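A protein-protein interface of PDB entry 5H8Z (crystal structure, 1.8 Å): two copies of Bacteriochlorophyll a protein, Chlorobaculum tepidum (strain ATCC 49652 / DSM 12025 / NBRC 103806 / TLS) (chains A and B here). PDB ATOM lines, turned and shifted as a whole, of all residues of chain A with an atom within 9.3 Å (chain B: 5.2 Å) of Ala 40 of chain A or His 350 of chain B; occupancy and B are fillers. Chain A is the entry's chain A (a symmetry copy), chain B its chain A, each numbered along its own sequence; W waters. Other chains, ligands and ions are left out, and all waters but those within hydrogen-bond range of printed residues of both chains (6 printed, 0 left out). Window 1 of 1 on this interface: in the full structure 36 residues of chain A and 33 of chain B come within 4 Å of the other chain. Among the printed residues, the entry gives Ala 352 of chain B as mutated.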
ATOM      1  N   THR A   9      -0.417  -0.788  19.858  1.00  0.00           N
ATOM      2  CA  THR A   9       0.214   0.199  18.993  1.00  0.00           C
ATOM      3  C   THR A   9       0.336   1.541  19.713  1.00  0.00           C
ATOM      4  O   THR A   9      -0.659   2.101  20.137  1.00  0.00           O
ATOM      5  CB  THR A   9      -0.606   0.387  17.732  1.00  0.00           C
ATOM      6  OG1 THR A   9      -0.813  -0.901  17.111  1.00  0.00           O
ATOM      7  CG2 THR A   9       0.100   1.295  16.770  1.00  0.00           C
ATOM      8  N   ASN A  36       4.897   1.790  16.260  1.00  0.00           N
ATOM      9  CA  ASN A  36       5.075   0.408  15.846  1.00  0.00           C
ATOM     10  C   ASN A  36       3.908  -0.004  14.974  1.00  0.00           C
ATOM     11  O   ASN A  36       3.142  -0.892  15.327  1.00  0.00           O
ATOM     12  CB  ASN A  36       5.212  -0.525  17.034  1.00  0.00           C
ATOM     13  CG  ASN A  36       4.047  -0.431  17.997  1.00  0.00           C
ATOM     14  OD1 ASN A  36       3.448   0.625  18.151  1.00  0.00           O
ATOM     15  ND2 ASN A  36       3.707  -1.558  18.642  1.00  0.00           N
ATOM     16  N   ALA A  37       3.773   0.670  13.834  1.00  0.00           N
ATOM     17  CA  ALA A  37       2.802   0.262  12.830  1.00  0.00           C
ATOM     18  C   ALA A  37       3.448   0.440  11.465  1.00  0.00           C
ATOM     19  O   ALA A  37       4.271   1.336  11.310  1.00  0.00           O
ATOM     20  CB  ALA A  37       1.507   1.132  12.942  1.00  0.00           C
ATOM     21  N   PRO A  38       3.031  -0.353  10.451  1.00  0.00           N
ATOM     22  CA  PRO A  38       3.708  -0.246   9.155  1.00  0.00           C
ATOM     23  C   PRO A  38       3.277   0.982   8.359  1.00  0.00           C
ATOM     24  O   PRO A  38       2.114   1.418   8.454  1.00  0.00           O
ATOM     25  CB  PRO A  38       3.277  -1.533   8.427  1.00  0.00           C
ATOM     26  CG  PRO A  38       1.908  -1.813   8.983  1.00  0.00           C
ATOM     27  CD  PRO A  38       1.973  -1.380  10.457  1.00  0.00           C
ATOM     28  N   PRO A  39       4.178   1.514   7.537  1.00  0.00           N
ATOM     29  CA  PRO A  39       3.771   2.552   6.581  1.00  0.00           C
ATOM     30  C   PRO A  39       2.901   1.941   5.487  1.00  0.00           C
ATOM     31  O   PRO A  39       2.920   0.704   5.281  1.00  0.00           O
ATOM     32  CB  PRO A  39       5.106   3.047   6.005  1.00  0.00           C
ATOM     33  CG  PRO A  39       6.007   1.842   6.144  1.00  0.00           C
ATOM     34  CD  PRO A  39       5.599   1.136   7.405  1.00  0.00           C
ATOM     35  N   ALA A  40       2.172   2.792   4.774  1.00  0.00           N
ATOM     36  CA  ALA A  40       1.343   2.358   3.645  1.00  0.00           C
ATOM     37  C   ALA A  40       2.155   2.413   2.337  1.00  0.00           C
ATOM     38  O   ALA A  40       1.682   2.924   1.326  1.00  0.00           O
ATOM     39  CB  ALA A  40       0.081   3.239   3.557  1.00  0.00           C
ATOM     40  N   SER A  41       3.384   1.894   2.368  1.00  0.00           N
ATOM     41  CA  SER A  41       4.181   1.757   1.143  1.00  0.00           C
ATOM     42  C   SER A  41       4.119   0.305   0.653  1.00  0.00           C
ATOM     43  O   SER A  41       4.370  -0.600   1.421  1.00  0.00           O
ATOM     44  CB  SER A  41       5.654   2.134   1.377  1.00  0.00           C
ATOM     45  OG  SER A  41       6.338   1.882   0.158  1.00  0.00           O
ATOM     46  N   PRO A  42       3.801   0.096  -0.631  1.00  0.00           N
ATOM     47  CA  PRO A  42       3.707  -1.287  -1.118  1.00  0.00           C
ATOM     48  C   PRO A  42       5.102  -1.864  -1.415  1.00  0.00           C
ATOM     49  O   PRO A  42       5.206  -3.018  -1.799  1.00  0.00           O
ATOM     50  CB  PRO A  42       2.843  -1.153  -2.370  1.00  0.00           C
ATOM     51  CG  PRO A  42       3.113   0.259  -2.878  1.00  0.00           C
ATOM     52  CD  PRO A  42       3.410   1.097  -1.643  1.00  0.00           C
ATOM     53  N   LEU A  43       6.158  -1.082  -1.156  1.00  0.00           N
ATOM     54  CA  LEU A  43       7.534  -1.604  -1.155  1.00  0.00           C
ATOM     55  C   LEU A  43       8.215  -1.223   0.166  1.00  0.00           C
ATOM     56  O   LEU A  43       8.201  -0.035   0.519  1.00  0.00           O
ATOM     57  CB  LEU A  43       8.317  -1.025  -2.345  1.00  0.00           C
ATOM     58  CG  LEU A  43       7.939  -1.627  -3.714  1.00  0.00           C
ATOM     59  CD1 LEU A  43       8.741  -0.889  -4.782  1.00  0.00           C
ATOM     60  CD2 LEU A  43       8.182  -3.152  -3.771  1.00  0.00           C
ATOM     61  N   LEU A  44       8.771  -2.215   0.877  1.00  0.00           N
ATOM     62  CA  LEU A  44       9.461  -2.020   2.148  1.00  0.00           C
ATOM     63  C   LEU A  44      10.781  -2.823   2.123  1.00  0.00           C
ATOM     64  O   LEU A  44      10.916  -3.759   1.335  1.00  0.00           O
ATOM     65  CB  LEU A  44       8.541  -2.452   3.320  1.00  0.00           C
ATOM     66  CG  LEU A  44       7.322  -1.532   3.488  1.00  0.00           C
ATOM     67  CD1 LEU A  44       6.335  -2.092   4.583  1.00  0.00           C
ATOM     68  CD2 LEU A  44       7.794  -0.088   3.845  1.00  0.00           C
ATOM     69  N   ALA A  46      11.640   1.150   3.585  1.00  0.00           N
ATOM     70  CA  ALA A  46      11.757   2.413   2.916  1.00  0.00           C
ATOM     71  C   ALA A  46      12.367   3.380   3.913  1.00  0.00           C
ATOM     72  O   ALA A  46      11.782   3.634   4.963  1.00  0.00           O
ATOM     73  CB  ALA A  46      10.391   2.916   2.437  1.00  0.00           C
ATOM     74  N   PRO A 187      -0.550   6.961  -5.515  1.00  0.00           N
ATOM     75  CA  PRO A 187      -1.533   7.706  -4.731  1.00  0.00           C
ATOM     76  C   PRO A 187      -1.304   9.215  -4.740  1.00  0.00           C
ATOM     77  O   PRO A 187      -2.095   9.943  -4.131  1.00  0.00           O
ATOM     78  CB  PRO A 187      -1.341   7.160  -3.304  1.00  0.00           C
ATOM     79  CG  PRO A 187       0.114   6.735  -3.250  1.00  0.00           C
ATOM     80  CD  PRO A 187       0.405   6.200  -4.671  1.00  0.00           C
ATOM     81  N   SER A 259      11.756   3.046   7.923  1.00  0.00           N
ATOM     82  CA  SER A 259      10.489   2.318   8.063  1.00  0.00           C
ATOM     83  C   SER A 259      10.556   0.930   7.463  1.00  0.00           C
ATOM     84  O   SER A 259      11.289   0.687   6.496  1.00  0.00           O
ATOM     85  CB  SER A 259       9.327   3.095   7.407  1.00  0.00           C
ATOM     86  OG  SER A 259       9.384   3.109   5.987  1.00  0.00           O
ATOM     87  N   ASP A 260       9.776   0.035   8.039  1.00  0.00           N
ATOM     88  CA  ASP A 260       9.651  -1.318   7.529  1.00  0.00           C
ATOM     89  C   ASP A 260       8.365  -1.912   8.052  1.00  0.00           C
ATOM     90  O   ASP A 260       7.530  -1.203   8.587  1.00  0.00           O
ATOM     91  CB  ASP A 260      10.834  -2.190   7.943  1.00  0.00           C
ATOM     92  CG  ASP A 260      11.046  -2.247   9.469  1.00  0.00           C
ATOM     93  OD1 ASP A 260      10.100  -2.051  10.266  1.00  0.00           O
ATOM     94  OD2 ASP A 260      12.200  -2.526   9.871  1.00  0.00           O
ATOM     95  N   SER A 261       8.207  -3.229   7.908  1.00  0.00           N
ATOM     96  CA  SER A 261       6.962  -3.876   8.282  1.00  0.00           C
ATOM     97  C   SER A 261       6.650  -3.717   9.778  1.00  0.00           C
ATOM     98  O   SER A 261       5.503  -3.857  10.188  1.00  0.00           O
ATOM     99  CB  SER A 261       7.005  -5.384   7.903  1.00  0.00           C
ATOM    100  OG  SER A 261       7.929  -6.037   8.743  1.00  0.00           O
ATOM    101  N   GLY A 263       7.469  -0.883  11.774  1.00  0.00           N
ATOM    102  CA  GLY A 263       7.209   0.470  12.264  1.00  0.00           C
ATOM    103  C   GLY A 263       7.886   1.586  11.501  1.00  0.00           C
ATOM    104  O   GLY A 263       8.458   1.393  10.431  1.00  0.00           O
ATOM    105  N   ILE A 264       7.778   2.783  12.066  1.00  0.00           N
ATOM    106  CA  ILE A 264       8.282   3.995  11.470  1.00  0.00           C
ATOM    107  C   ILE A 264       8.989   4.801  12.553  1.00  0.00           C
ATOM    108  O   ILE A 264       8.470   4.902  13.665  1.00  0.00           O
ATOM    109  CB  ILE A 264       7.134   4.864  10.905  1.00  0.00           C
ATOM    110  CG1 ILE A 264       6.268   4.037   9.960  1.00  0.00           C
ATOM    111  CG2 ILE A 264       7.711   6.114  10.228  1.00  0.00           C
ATOM    112  CD1 ILE A 264       4.958   4.724   9.488  1.00  0.00           C
ATOM    113  N   HIS A 296      -2.704  15.484   3.639  1.00  0.00           N
ATOM    114  CA  HIS A 296      -2.015  14.431   2.920  1.00  0.00           C
ATOM    115  C   HIS A 296      -1.631  13.298   3.858  1.00  0.00           C
ATOM    116  O   HIS A 296      -1.847  12.158   3.550  1.00  0.00           O
ATOM    117  CB  HIS A 296      -0.821  14.949   2.147  1.00  0.00           C
ATOM    118  CG  HIS A 296      -1.179  15.704   0.916  1.00  0.00           C
ATOM    119  ND1 HIS A 296      -0.253  16.078  -0.016  1.00  0.00           N
ATOM    120  CD2 HIS A 296      -2.358  16.160   0.463  1.00  0.00           C
ATOM    121  CE1 HIS A 296      -0.837  16.742  -0.978  1.00  0.00           C
ATOM    122  NE2 HIS A 296      -2.121  16.787  -0.726  1.00  0.00           N
ATOM    123  N   HIS A 297      -1.058  13.630   4.996  1.00  0.00           N
ATOM    124  CA  HIS A 297      -0.707  12.596   5.951  1.00  0.00           C
ATOM    125  C   HIS A 297      -1.987  11.898   6.450  1.00  0.00           C
ATOM    126  O   HIS A 297      -1.950  10.800   6.844  1.00  0.00           O
ATOM    127  CB  HIS A 297       0.091  13.124   7.108  1.00  0.00           C
ATOM    128  CG  HIS A 297       0.518  12.077   8.079  1.00  0.00           C
ATOM    129  ND1 HIS A 297      -0.265  11.669   9.113  1.00  0.00           N
ATOM    130  CD2 HIS A 297       1.648  11.351   8.163  1.00  0.00           C
ATOM    131  CE1 HIS A 297       0.360  10.746   9.798  1.00  0.00           C
ATOM    132  NE2 HIS A 297       1.523  10.538   9.247  1.00  0.00           N
ATOM    133  N   GLY A 298      -3.107  12.585   6.428  1.00  0.00           N
ATOM    134  CA  GLY A 298      -4.370  12.036   6.851  1.00  0.00           C
ATOM    135  C   GLY A 298      -4.743  10.787   6.021  1.00  0.00           C
ATOM    136  O   GLY A 298      -5.404   9.886   6.477  1.00  0.00           O
ATOM    137  N   MET A 299      -4.268  10.774   4.787  1.00  0.00           N
ATOM    138  CA  MET A 299      -4.484   9.642   3.895  1.00  0.00           C
ATOM    139  C   MET A 299      -3.749   8.380   4.360  1.00  0.00           C
ATOM    140  O   MET A 299      -4.060   7.313   3.874  1.00  0.00           O
ATOM    141  CB  MET A 299      -4.063  10.028   2.461  1.00  0.00           C
ATOM    142  CG  MET A 299      -4.815  11.284   1.960  1.00  0.00           C
ATOM    143  SD  MET A 299      -4.279  11.784   0.310  1.00  0.00           S
ATOM    144  CE  MET A 299      -4.969  10.457  -0.647  1.00  0.00           C
ATOM    145  N   VAL A 300      -2.787   8.483   5.285  1.00  0.00           N
ATOM    146  CA  VAL A 300      -2.087   7.289   5.790  1.00  0.00           C
ATOM    147  C   VAL A 300      -2.246   7.073   7.297  1.00  0.00           C
ATOM    148  O   VAL A 300      -1.920   6.014   7.784  1.00  0.00           O
ATOM    149  CB  VAL A 300      -0.536   7.309   5.447  1.00  0.00           C
ATOM    150  CG1 VAL A 300      -0.342   7.285   3.942  1.00  0.00           C
ATOM    151  CG2 VAL A 300       0.186   8.529   6.056  1.00  0.00           C
ATOM    152  N   GLY A 301      -2.770   8.061   8.026  1.00  0.00           N
ATOM    153  CA  GLY A 301      -2.773   8.013   9.489  1.00  0.00           C
ATOM    154  C   GLY A 301      -3.898   7.267  10.169  1.00  0.00           C
ATOM    155  O   GLY A 301      -3.944   7.226  11.405  1.00  0.00           O
ATOM    156  N   LYS A 302      -4.764   6.634   9.372  1.00  0.00           N
ATOM    157  CA  LYS A 302      -5.968   6.017   9.889  1.00  0.00           C
ATOM    158  C   LYS A 302      -5.988   4.482   9.811  1.00  0.00           C
ATOM    159  O   LYS A 302      -7.030   3.882  10.089  1.00  0.00           O
ATOM    160  CB  LYS A 302      -7.218   6.548   9.147  1.00  0.00           C
ATOM    161  CG  LYS A 302      -7.452   8.060   9.211  1.00  0.00           C
ATOM    162  CD  LYS A 302      -8.844   8.336   8.570  1.00  0.00           C
ATOM    163  CE  LYS A 302      -9.126   9.813   8.327  1.00  0.00           C
ATOM    164  NZ  LYS A 302      -8.169  10.388   7.290  1.00  0.00           N
ATOM    165  N   PHE A 303      -4.858   3.836   9.512  1.00  0.00           N
ATOM    166  CA  PHE A 303      -4.899   2.397   9.261  1.00  0.00           C
ATOM    167  C   PHE A 303      -4.615   1.513  10.467  1.00  0.00           C
ATOM    168  O   PHE A 303      -4.933   0.327  10.426  1.00  0.00           O
ATOM    169  CB  PHE A 303      -3.903   2.066   8.147  1.00  0.00           C
ATOM    170  CG  PHE A 303      -4.193   2.762   6.842  1.00  0.00           C
ATOM    171  CD1 PHE A 303      -5.517   2.876   6.323  1.00  0.00           C
ATOM    172  CD2 PHE A 303      -3.153   3.326   6.133  1.00  0.00           C
ATOM    173  CE1 PHE A 303      -5.715   3.488   5.077  1.00  0.00           C
ATOM    174  CE2 PHE A 303      -3.354   3.956   4.901  1.00  0.00           C
ATOM    175  CZ  PHE A 303      -4.633   4.042   4.381  1.00  0.00           C
ATOM    176  N   ASN A 304      -4.062   2.069  11.541  1.00  0.00           N
ATOM    177  CA  ASN A 304      -3.908   1.310  12.810  1.00  0.00           C
ATOM    178  C   ASN A 304      -4.263   2.183  13.983  1.00  0.00           C
ATOM    179  O   ASN A 304      -3.743   3.289  14.093  1.00  0.00           O
ATOM    180  CB  ASN A 304      -2.469   0.794  13.019  1.00  0.00           C
ATOM    181  CG  ASN A 304      -2.126  -0.388  12.102  1.00  0.00           C
ATOM    182  OD1 ASN A 304      -2.583  -1.530  12.328  1.00  0.00           O
ATOM    183  ND2 ASN A 304      -1.364  -0.123  11.068  1.00  0.00           N
ATOM    184  N   ASN A 305      -5.136   1.684  14.855  1.00  0.00           N
ATOM    185  CA  ASN A 305      -5.421   2.372  16.126  1.00  0.00           C
ATOM    186  C   ASN A 305      -4.141   2.573  16.904  1.00  0.00           C
ATOM    187  O   ASN A 305      -3.276   1.727  16.883  1.00  0.00           O
ATOM    188  CB  ASN A 305      -6.394   1.566  16.993  1.00  0.00           C
ATOM    189  CG  ASN A 305      -7.832   1.770  16.606  1.00  0.00           C
ATOM    190  OD1 ASN A 305      -8.183   2.752  15.962  1.00  0.00           O
ATOM    191  ND2 ASN A 305      -8.688   0.836  17.015  1.00  0.00           N
ATOM    192  N   ALA B 345      -1.317  -9.555  13.018  1.00  0.00           N
ATOM    193  CA  ALA B 345      -2.628  -8.983  13.333  1.00  0.00           C
ATOM    194  C   ALA B 345      -2.661  -7.496  13.023  1.00  0.00           C
ATOM    195  O   ALA B 345      -3.664  -6.963  12.563  1.00  0.00           O
ATOM    196  CB  ALA B 345      -2.970  -9.214  14.814  1.00  0.00           C
ATOM    197  N   ARG B 346      -1.553  -6.823  13.300  1.00  0.00           N
ATOM    198  CA  ARG B 346      -1.464  -5.400  13.046  1.00  0.00           C
ATOM    199  C   ARG B 346      -1.498  -5.100  11.543  1.00  0.00           C
ATOM    200  O   ARG B 346      -2.077  -4.108  11.087  1.00  0.00           O
ATOM    201  CB  ARG B 346      -0.192  -4.845  13.694  1.00  0.00           C
ATOM    202  CG  ARG B 346      -0.105  -3.393  13.620  1.00  0.00           C
ATOM    203  CD  ARG B 346       1.015  -2.865  14.467  1.00  0.00           C
ATOM    204  NE  ARG B 346       0.824  -3.111  15.887  1.00  0.00           N
ATOM    205  CZ  ARG B 346       1.616  -3.900  16.601  1.00  0.00           C
ATOM    206  NH1 ARG B 346       2.633  -4.526  16.010  1.00  0.00           N
ATOM    207  NH2 ARG B 346       1.386  -4.074  17.895  1.00  0.00           N
ATOM    208  N   TRP B 347      -0.861  -5.965  10.765  1.00  0.00           N
ATOM    209  CA  TRP B 347      -0.899  -5.792   9.320  1.00  0.00           C
ATOM    210  C   TRP B 347      -2.343  -6.051   8.804  1.00  0.00           C
ATOM    211  O   TRP B 347      -2.814  -5.352   7.909  1.00  0.00           O
ATOM    212  CB  TRP B 347       0.141  -6.725   8.637  1.00  0.00           C
ATOM    213  CG  TRP B 347       0.087  -6.654   7.137  1.00  0.00           C
ATOM    214  CD1 TRP B 347       0.671  -5.725   6.340  1.00  0.00           C
ATOM    215  CD2 TRP B 347      -0.628  -7.542   6.277  1.00  0.00           C
ATOM    216  NE1 TRP B 347       0.356  -5.974   5.006  1.00  0.00           N
ATOM    217  CE2 TRP B 347      -0.442  -7.091   4.954  1.00  0.00           C
ATOM    218  CE3 TRP B 347      -1.421  -8.680   6.507  1.00  0.00           C
ATOM    219  CZ2 TRP B 347      -1.013  -7.753   3.836  1.00  0.00           C
ATOM    220  CZ3 TRP B 347      -1.990  -9.330   5.398  1.00  0.00           C
ATOM    221  CH2 TRP B 347      -1.806  -8.837   4.093  1.00  0.00           C
ATOM    222  N   VAL B 348      -3.046  -7.049   9.358  1.00  0.00           N
ATOM    223  CA  VAL B 348      -4.432  -7.315   8.945  1.00  0.00           C
ATOM    224  C   VAL B 348      -5.308  -6.102   9.213  1.00  0.00           C
ATOM    225  O   VAL B 348      -6.056  -5.692   8.326  1.00  0.00           O
ATOM    226  CB  VAL B 348      -5.015  -8.532   9.653  1.00  0.00           C
ATOM    227  CG1 VAL B 348      -6.500  -8.697   9.342  1.00  0.00           C
ATOM    228  CG2 VAL B 348      -4.242  -9.754   9.167  1.00  0.00           C
ATOM    229  N   GLU B 349      -5.168  -5.517  10.405  1.00  0.00           N
ATOM    230  CA  GLU B 349      -5.888  -4.256  10.703  1.00  0.00           C
ATOM    231  C   GLU B 349      -5.565  -3.182   9.656  1.00  0.00           C
ATOM    232  O   GLU B 349      -6.486  -2.548   9.074  1.00  0.00           O
ATOM    233  CB  GLU B 349      -5.546  -3.748  12.121  1.00  0.00           C
ATOM    234  CG  GLU B 349      -6.242  -2.414  12.432  1.00  0.00           C
ATOM    235  CD  GLU B 349      -5.761  -1.738  13.701  1.00  0.00           C
ATOM    236  OE1 GLU B 349      -4.720  -2.157  14.245  1.00  0.00           O
ATOM    237  OE2 GLU B 349      -6.429  -0.756  14.124  1.00  0.00           O
ATOM    238  N   HIS B 350      -4.273  -2.995   9.398  1.00  0.00           N
ATOM    239  CA  HIS B 350      -3.806  -1.995   8.425  1.00  0.00           C
ATOM    240  C   HIS B 350      -4.438  -2.172   7.056  1.00  0.00           C
ATOM    241  O   HIS B 350      -5.057  -1.247   6.526  1.00  0.00           O
ATOM    242  CB  HIS B 350      -2.278  -2.096   8.370  1.00  0.00           C
ATOM    243  CG  HIS B 350      -1.585  -1.282   7.309  1.00  0.00           C
ATOM    244  ND1 HIS B 350      -1.148   0.009   7.502  1.00  0.00           N
ATOM    245  CD2 HIS B 350      -1.157  -1.632   6.072  1.00  0.00           C
ATOM    246  CE1 HIS B 350      -0.490   0.427   6.425  1.00  0.00           C
ATOM    247  NE2 HIS B 350      -0.494  -0.545   5.539  1.00  0.00           N
ATOM    248  N   VAL B 351      -4.376  -3.390   6.494  1.00  0.00           N
ATOM    249  CA  VAL B 351      -4.902  -3.554   5.136  1.00  0.00           C
ATOM    250  C   VAL B 351      -6.426  -3.553   5.104  1.00  0.00           C
ATOM    251  O   VAL B 351      -7.003  -3.101   4.116  1.00  0.00           O
ATOM    252  CB  VAL B 351      -4.380  -4.844   4.423  1.00  0.00           C
ATOM    253  CG1 VAL B 351      -2.848  -4.742   4.292  1.00  0.00           C
ATOM    254  CG2 VAL B 351      -4.775  -6.163   5.176  1.00  0.00           C
ATOM    255  N   ALA B 352      -7.069  -4.002   6.178  1.00  0.00           N
ATOM    256  CA  ALA B 352      -8.550  -3.996   6.212  1.00  0.00           C
ATOM    257  C   ALA B 352      -9.081  -2.559   6.232  1.00  0.00           C
ATOM    258  O   ALA B 352     -10.223  -2.322   5.839  1.00  0.00           O
ATOM    259  CB  ALA B 352      -9.095  -4.773   7.425  1.00  0.00           C
ATOM    260  N   LYS B 353      -8.263  -1.606   6.692  1.00  0.00           N
ATOM    261  CA  LYS B 353      -8.708  -0.212   6.777  1.00  0.00           C
ATOM    262  C   LYS B 353      -8.263   0.589   5.563  1.00  0.00           C
ATOM    263  O   LYS B 353      -8.601   1.769   5.435  1.00  0.00           O
ATOM    264  CB  LYS B 353      -8.168   0.467   8.064  1.00  0.00           C
ATOM    265  CG  LYS B 353      -8.841  -0.083   9.345  1.00  0.00           C
ATOM    266  CD  LYS B 353      -8.264   0.601  10.614  1.00  0.00           C
ATOM    267  CE  LYS B 353      -8.979   0.138  11.892  1.00  0.00           C
ATOM    268  NZ  LYS B 353      -8.384   0.849  13.066  1.00  0.00           N
ATOM    269  N   GLY B 354      -7.494  -0.046   4.678  1.00  0.00           N
ATOM    270  CA  GLY B 354      -7.111   0.582   3.412  1.00  0.00           C
ATOM    271  C   GLY B 354      -5.608   0.759   3.182  1.00  0.00           C
ATOM    272  O   GLY B 354      -5.190   1.342   2.159  1.00  0.00           O
ATOM    273  N   GLY B 355      -4.798   0.286   4.124  1.00  0.00           N
ATOM    274  CA  GLY B 355      -3.357   0.423   3.997  1.00  0.00           C
ATOM    275  C   GLY B 355      -2.832  -0.593   3.000  1.00  0.00           C
ATOM    276  O   GLY B 355      -3.438  -1.669   2.838  1.00  0.00           O
ATOM    277  N   VAL B 356      -1.711  -0.269   2.352  1.00  0.00           N
ATOM    278  CA  VAL B 356      -1.106  -1.172   1.372  1.00  0.00           C
ATOM    279  C   VAL B 356       0.355  -1.513   1.697  1.00  0.00           C
ATOM    280  O   VAL B 356       1.107  -1.952   0.809  1.00  0.00           O
ATOM    281  CB  VAL B 356      -1.188  -0.585  -0.057  1.00  0.00           C
ATOM    282  CG1 VAL B 356      -2.643  -0.371  -0.457  1.00  0.00           C
ATOM    283  CG2 VAL B 356      -0.408   0.743  -0.229  1.00  0.00           C
ATOM    284  N   GLY B 357       0.740  -1.320   2.947  1.00  0.00           N
ATOM    285  CA  GLY B 357       2.074  -1.706   3.420  1.00  0.00           C
ATOM    286  C   GLY B 357       2.387  -3.138   3.024  1.00  0.00           C
ATOM    287  O   GLY B 357       1.539  -4.029   3.164  1.00  0.00           O
HETATM  288  O   HOH W   1      -7.420   3.515  13.113  1.00  0.00           O
HETATM  289  O   HOH W   2      -0.393   1.967   9.636  1.00  0.00           O
HETATM  290  O   HOH W   3       2.452  -4.982  11.306  1.00  0.00           O
HETATM  291  O   HOH W   4      -3.418  -0.871  16.323  1.00  0.00           O
HETATM  292  O   HOH W   5       3.971  -3.899  13.328  1.00  0.00           O
HETATM  293  O   HOH W   6      -9.340  -1.467  14.560  1.00  0.00           O
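NE of Arg 346 of chain B is in hydrogen-bond range of OG1 of Thr 9 of chain A.
O of Asn 36 of chain A lies close to NE of Arg 346 of chain B, 3.3 Å away.
The backbone carbonyl oxygen (O) of Arg 346 of chain B sits close to the side-chain amide oxygen (OD1) of Asn 304 of chain A.
OE1 of Glu 349 of chain B lies close to OD1 of Asn 304 of chain A, 2.9 Å away.
The backbone NH (N) of Asn 305 of chain A lies within hydrogen-bond range of the side-chain carboxylate (OE2) of Glu 349 of chain B (2.9 Å).
The side-chain amino group (NZ) of Lys 353 of chain B is in hydrogen-bond range of the side-chain amide oxygen (OD1) of Asn 305 of chain A (3.5 Å).
The indole nitrogen of Trp 347 of chain B is in hydrogen-bond range of the backbone carbonyl oxygen of Gly 357 of chain B, 2.9 Å away.
OE2 of Glu 349 of chain B is in salt-bridge range of NZ of Lys 353 of chain B.
The backbone carbonyl oxygen (O) of His 350 of chain B sits at hydrogen-bond distance from the backbone NH (N) of Gly 355 of chain B, 2.9 Å away.
O of Gly 298 of chain A is in hydrogen-bond range of NZ of Lys 302 of chain A, 2.9 Å away.
Among the printed residues, merely in contact across the chains: Pro 39 of chain A with Gly 357 of chain B (3.2 Å), Ser 41 of chain A with Gly 357 of chain B (3.2 Å), Phe 303 of chain A with His 350 of chain B (3.3 Å), Pro 42 of chain A with Val 356 of chain B (3.3 Å), Phe 303 of chain A with Gly 354 of chain B (3.3 Å), Phe 303 of chain A with Lys 353 of chain B (3.3 Å), Ala 40 of chain A with Val 356 of chain B (3.4 Å), Pro 38 of chain A with His 350 of chain B (3.4 Å), Phe 303 of chain A with Gly 355 of chain B (3.5 Å), Asn 304 of chain A with His 350 of chain B (3.5 Å), Phe 303 of chain A with Glu 349 of chain B (3.5 Å), Lys 302 of chain A with Lys 353 of chain B (3.5 Å), Ser 41 of chain A with Val 356 of chain B (3.6 Å), Pro 39 of chain A with His 350 of chain B (3.6 Å), Ala 40 of chain A with Gly 357 of chain B (3.8 Å), Ala 40 of chain A with His 350 of chain B (3.8 Å) and Ala 37 of chain A with Arg 346 of chain B (3.96 Å).
Printed residues of chain B within 4 Å of Asn 36 of chain A: Arg 346.
Of the printed residues of chain B, Pro 38 of chain A touches His 350.
Of the printed residues of chain B, Ala 40 of chain A touches His 350, Val 356 and Gly 357.
Of the printed residues of chain B, Lys 302 of chain A touches Lys 353.
Printed residues of chain B within 4 Å of Phe 303 of chain A: Glu 349, His 350, Lys 353, Gly 354 and Gly 355.
Trp 347 of chain B touches none of the printed residues of chain A.
His 350 of chain B touches just these residues of chain A: Pro 38 (3.4 Å), Pro 39 (3.6 Å), Ala 40 (3.8 Å), Phe 303 (3.3 Å) and Asn 304 (3.5 Å).
No residue of chain A comes within 4 Å of Val 351 of chain B.
Of chain A, only Pro 39 (3.2 Å), Ala 40 (3.8 Å) and Ser 41 (3.2 Å) come within 4 Å of Gly 357 of chain B.
Of the 13 printed residues of chain B, 8 touch a printed residue of chain A.
Along chain B the printed residues that touch a printed residue of chain A span positions 346 to 357.
Of the 27 printed residues of chain A, 12 touch a printed residue of chain B.
Printed residues of chain A that touch a printed residue of chain B: Thr 9, Asn 36, Ala 37, Pro 38, Pro 39, Ala 40, Ser 41, Pro 42, Lys 302, Phe 303, Asn 304 and Asn 305.
Hydrophobic or aromatic side chains of chain A within 4 Å of the printed part of chain B: Pro 38, Pro 42 and Phe 303.
Among the printed residues, no Asp or Glu carboxylate lies within 4 Å of a Lys or Arg side-chain nitrogen of the other chain.
No position is printed for both chains.
Of the 23 pairs that touch across the chains among the printed residues, none has its exchanged pair printed and touching as well.
Water W4 lies within hydrogen-bond range of O of Asn 305 of chain A (2.7 Å), OG1 of Thr 9 of chain A (2.7 Å) and OE1 of Glu 349 of chain B (2.8 Å).
Water W6 lies within hydrogen-bond range of NZ of Lys 353 of chain B, OE2 of Glu 349 of chain B and ND2 of Asn 305 of chain A.
Water W3 bridges the backbone carbonyl oxygen (O) of Ser 261 of chain A and the backbone NH (N) of Trp 347 of chain B.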
